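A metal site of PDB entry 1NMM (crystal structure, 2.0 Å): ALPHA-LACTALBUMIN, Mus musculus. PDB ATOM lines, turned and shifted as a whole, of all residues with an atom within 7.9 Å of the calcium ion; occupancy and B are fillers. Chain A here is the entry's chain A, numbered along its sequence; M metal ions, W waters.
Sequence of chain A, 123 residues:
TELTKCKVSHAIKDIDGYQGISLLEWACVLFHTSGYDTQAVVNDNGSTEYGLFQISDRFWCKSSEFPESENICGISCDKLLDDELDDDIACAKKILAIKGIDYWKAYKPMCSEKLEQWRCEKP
The calcium ion is bound by O of Glu 84 (2.2 Å), OD1 of Asp 87 (2.4 Å), O of Lys 79 (2.4 Å), OD2 of Asp 88 (2.4 Å), water W2 (2.5 Å), OD1 of Asp 82 (2.5 Å) and water W1 (2.6 Å). The calcium ion has seven donor atoms within binding distance.
Water W1 lies within hydrogen-bond range of the side-chain carboxylate of Asp 87 (2.6 Å) and the side-chain carboxylate of Asp 82 (2.7 Å).
Within 4 Å of the calcium ion: Lys 79, Asp 82, Glu 84, Asp 87 and Asp 88. Along chain A the residues within 4 Å of the calcium ion span positions 79 to 88.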
ATOM      1  N   THR A  38       8.134   3.195   0.210  1.00  0.00           N
ATOM      2  CA  THR A  38       8.513   4.089  -0.884  1.00  0.00           C
ATOM      3  C   THR A  38       9.804   3.728  -1.585  1.00  0.00           C
ATOM      4  O   THR A  38      10.081   4.277  -2.666  1.00  0.00           O
ATOM      5  CB  THR A  38       8.714   5.500  -0.397  1.00  0.00           C
ATOM      6  OG1 THR A  38       9.724   5.491   0.611  1.00  0.00           O
ATOM      7  CG2 THR A  38       7.408   6.086   0.134  1.00  0.00           C
ATOM      8  N   ILE A  75      10.738  10.120 -16.745  1.00  0.00           N
ATOM      9  CA  ILE A  75      11.343  10.281 -15.449  1.00  0.00           C
ATOM     10  C   ILE A  75      12.312   9.177 -15.103  1.00  0.00           C
ATOM     11  O   ILE A  75      12.183   8.039 -15.557  1.00  0.00           O
ATOM     12  CB  ILE A  75      10.235  10.372 -14.380  1.00  0.00           C
ATOM     13  CG1 ILE A  75      10.794  10.935 -13.081  1.00  0.00           C
ATOM     14  CG2 ILE A  75       9.622   8.981 -14.142  1.00  0.00           C
ATOM     15  CD1 ILE A  75       9.745  11.040 -11.977  1.00  0.00           C
ATOM     16  N   SER A  76      13.324   9.513 -14.300  1.00  0.00           N
ATOM     17  CA  SER A  76      14.300   8.528 -13.898  1.00  0.00           C
ATOM     18  C   SER A  76      13.620   7.654 -12.855  1.00  0.00           C
ATOM     19  O   SER A  76      12.921   8.182 -11.971  1.00  0.00           O
ATOM     20  CB  SER A  76      15.507   9.207 -13.258  1.00  0.00           C
ATOM     21  OG  SER A  76      16.292   8.234 -12.587  1.00  0.00           O
ATOM     22  N   CYS A  77      13.811   6.349 -12.926  1.00  0.00           N
ATOM     23  CA  CYS A  77      13.187   5.489 -11.925  1.00  0.00           C
ATOM     24  C   CYS A  77      13.650   5.821 -10.488  1.00  0.00           C
ATOM     25  O   CYS A  77      12.934   5.552  -9.532  1.00  0.00           O
ATOM     26  CB  CYS A  77      13.450   4.010 -12.270  1.00  0.00           C
ATOM     27  SG  CYS A  77      12.905   3.419 -13.938  1.00  0.00           S
ATOM     28  N   ASP A  78      14.841   6.419 -10.317  1.00  0.00           N
ATOM     29  CA  ASP A  78      15.306   6.768  -8.977  1.00  0.00           C
ATOM     30  C   ASP A  78      14.432   7.832  -8.307  1.00  0.00           C
ATOM     31  O   ASP A  78      14.403   7.951  -7.088  1.00  0.00           O
ATOM     32  CB  ASP A  78      16.763   7.231  -9.002  1.00  0.00           C
ATOM     33  CG  ASP A  78      17.716   6.143  -9.505  1.00  0.00           C
ATOM     34  OD1 ASP A  78      17.586   4.978  -9.085  1.00  0.00           O
ATOM     35  OD2 ASP A  78      18.602   6.455 -10.318  1.00  0.00           O
ATOM     36  N   LYS A  79      13.697   8.597  -9.106  1.00  0.00           N
ATOM     37  CA  LYS A  79      12.782   9.608  -8.576  1.00  0.00           C
ATOM     38  C   LYS A  79      11.560   8.947  -7.911  1.00  0.00           C
ATOM     39  O   LYS A  79      10.763   9.610  -7.254  1.00  0.00           O
ATOM     40  CB  LYS A  79      12.292  10.515  -9.707  1.00  0.00           C
ATOM     41  CG  LYS A  79      13.357  11.485 -10.238  1.00  0.00           C
ATOM     42  CD  LYS A  79      13.603  12.567  -9.201  1.00  0.00           C
ATOM     43  CE  LYS A  79      14.478  13.680  -9.749  1.00  0.00           C
ATOM     44  NZ  LYS A  79      14.430  14.862  -8.844  1.00  0.00           N
ATOM     45  N   LEU A  80      11.446   7.636  -8.084  1.00  0.00           N
ATOM     46  CA  LEU A  80      10.316   6.878  -7.528  1.00  0.00           C
ATOM     47  C   LEU A  80      10.725   6.151  -6.233  1.00  0.00           C
ATOM     48  O   LEU A  80       9.940   5.392  -5.664  1.00  0.00           O
ATOM     49  CB  LEU A  80       9.814   5.857  -8.563  1.00  0.00           C
ATOM     50  CG  LEU A  80       9.349   6.450  -9.909  1.00  0.00           C
ATOM     51  CD1 LEU A  80       9.004   5.318 -10.899  1.00  0.00           C
ATOM     52  CD2 LEU A  80       8.141   7.363  -9.690  1.00  0.00           C
ATOM     53  N   LEU A  81      11.954   6.397  -5.788  1.00  0.00           N
ATOM     54  CA  LEU A  81      12.451   5.781  -4.557  1.00  0.00           C
ATOM     55  C   LEU A  81      12.614   6.761  -3.389  1.00  0.00           C
ATOM     56  O   LEU A  81      13.326   6.471  -2.435  1.00  0.00           O
ATOM     57  CB  LEU A  81      13.767   5.030  -4.811  1.00  0.00           C
ATOM     58  CG  LEU A  81      13.698   3.924  -5.885  1.00  0.00           C
ATOM     59  CD1 LEU A  81      15.048   3.184  -6.000  1.00  0.00           C
ATOM     60  CD2 LEU A  81      12.575   2.941  -5.519  1.00  0.00           C
ATOM     61  N   ASP A  82      11.938   7.908  -3.434  1.00  0.00           N
ATOM     62  CA  ASP A  82      12.037   8.880  -2.335  1.00  0.00           C
ATOM     63  C   ASP A  82      10.650   9.094  -1.688  1.00  0.00           C
ATOM     64  O   ASP A  82       9.696   8.399  -2.019  1.00  0.00           O
ATOM     65  CB  ASP A  82      12.590  10.210  -2.866  1.00  0.00           C
ATOM     66  CG  ASP A  82      11.735  10.804  -3.980  1.00  0.00           C
ATOM     67  OD1 ASP A  82      10.484  10.769  -3.844  1.00  0.00           O
ATOM     68  OD2 ASP A  82      12.318  11.312  -4.980  1.00  0.00           O
ATOM     69  N   ASP A  83      10.541  10.044  -0.768  1.00  0.00           N
ATOM     70  CA  ASP A  83       9.275  10.275  -0.107  1.00  0.00           C
ATOM     71  C   ASP A  83       8.445  11.418  -0.681  1.00  0.00           C
ATOM     72  O   ASP A  83       7.482  11.844  -0.048  1.00  0.00           O
ATOM     73  CB  ASP A  83       9.481  10.492   1.391  1.00  0.00           C
ATOM     74  CG  ASP A  83      10.139   9.314   2.055  1.00  0.00           C
ATOM     75  OD1 ASP A  83      10.041   8.186   1.503  1.00  0.00           O
ATOM     76  OD2 ASP A  83      10.755   9.509   3.119  1.00  0.00           O
ATOM     77  N   GLU A  84       8.820  11.918  -1.857  1.00  0.00           N
ATOM     78  CA  GLU A  84       8.056  12.985  -2.491  1.00  0.00           C
ATOM     79  C   GLU A  84       7.245  12.228  -3.531  1.00  0.00           C
ATOM     80  O   GLU A  84       7.773  11.772  -4.555  1.00  0.00           O
ATOM     81  CB  GLU A  84       8.992  14.013  -3.134  1.00  0.00           C
ATOM     82  CG  GLU A  84       9.622  14.915  -2.087  1.00  0.00           C
ATOM     83  CD  GLU A  84      10.957  15.526  -2.523  1.00  0.00           C
ATOM     84  OE1 GLU A  84      10.979  16.325  -3.497  1.00  0.00           O
ATOM     85  OE2 GLU A  84      11.966  15.193  -1.877  1.00  0.00           O
ATOM     86  N   LEU A  85       5.970  12.093  -3.231  1.00  0.00           N
ATOM     87  CA  LEU A  85       5.046  11.309  -4.029  1.00  0.00           C
ATOM     88  C   LEU A  85       4.361  11.985  -5.214  1.00  0.00           C
ATOM     89  O   LEU A  85       3.643  11.328  -5.977  1.00  0.00           O
ATOM     90  CB  LEU A  85       4.015  10.695  -3.081  1.00  0.00           C
ATOM     91  CG  LEU A  85       4.280   9.318  -2.440  1.00  0.00           C
ATOM     92  CD1 LEU A  85       5.708   8.863  -2.586  1.00  0.00           C
ATOM     93  CD2 LEU A  85       3.859   9.369  -1.003  1.00  0.00           C
ATOM     94  N   ASP A  86       4.585  13.288  -5.408  1.00  0.00           N
ATOM     95  CA  ASP A  86       3.954  13.974  -6.535  1.00  0.00           C
ATOM     96  C   ASP A  86       4.266  13.369  -7.914  1.00  0.00           C
ATOM     97  O   ASP A  86       3.348  13.221  -8.733  1.00  0.00           O
ATOM     98  CB  ASP A  86       4.314  15.468  -6.525  1.00  0.00           C
ATOM     99  CG  ASP A  86       3.588  16.228  -5.411  1.00  0.00           C
ATOM    100  OD1 ASP A  86       3.771  15.854  -4.225  1.00  0.00           O
ATOM    101  OD2 ASP A  86       2.861  17.189  -5.701  1.00  0.00           O
ATOM    102  N   ASP A  87       5.520  13.022  -8.168  1.00  0.00           N
ATOM    103  CA  ASP A  87       5.863  12.442  -9.453  1.00  0.00           C
ATOM    104  C   ASP A  87       5.469  10.958  -9.556  1.00  0.00           C
ATOM    105  O   ASP A  87       5.189  10.478 -10.663  1.00  0.00           O
ATOM    106  CB  ASP A  87       7.359  12.631  -9.788  1.00  0.00           C
ATOM    107  CG  ASP A  87       8.283  12.259  -8.638  1.00  0.00           C
ATOM    108  OD1 ASP A  87       7.828  11.702  -7.614  1.00  0.00           O
ATOM    109  OD2 ASP A  87       9.500  12.519  -8.787  1.00  0.00           O
ATOM    110  N   ASP A  88       5.435  10.247  -8.434  1.00  0.00           N
ATOM    111  CA  ASP A  88       5.004   8.847  -8.445  1.00  0.00           C
ATOM    112  C   ASP A  88       3.539   8.856  -8.850  1.00  0.00           C
ATOM    113  O   ASP A  88       3.102   8.048  -9.677  1.00  0.00           O
ATOM    114  CB  ASP A  88       5.111   8.195  -7.061  1.00  0.00           C
ATOM    115  CG  ASP A  88       6.529   8.193  -6.529  1.00  0.00           C
ATOM    116  OD1 ASP A  88       7.066   7.112  -6.196  1.00  0.00           O
ATOM    117  OD2 ASP A  88       7.092   9.299  -6.455  1.00  0.00           O
ATOM    118  N   ILE A  89       2.808   9.781  -8.256  1.00  0.00           N
ATOM    119  CA  ILE A  89       1.379   9.939  -8.496  1.00  0.00           C
ATOM    120  C   ILE A  89       1.137  10.367  -9.942  1.00  0.00           C
ATOM    121  O   ILE A  89       0.266   9.826 -10.614  1.00  0.00           O
ATOM    122  CB  ILE A  89       0.756  10.978  -7.507  1.00  0.00           C
ATOM    123  CG1 ILE A  89       0.836  10.446  -6.073  1.00  0.00           C
ATOM    124  CG2 ILE A  89      -0.680  11.265  -7.865  1.00  0.00           C
ATOM    125  CD1 ILE A  89       0.522  11.509  -5.001  1.00  0.00           C
HETATM  126 CA    CA M   1       9.043  10.562  -5.929  1.00  0.00          CA
HETATM  127  O   HOH W   1      10.480  12.629  -6.401  1.00  0.00           O
HETATM  128  O   HOH W   2       9.064   8.332  -4.836  1.00  0.00           O
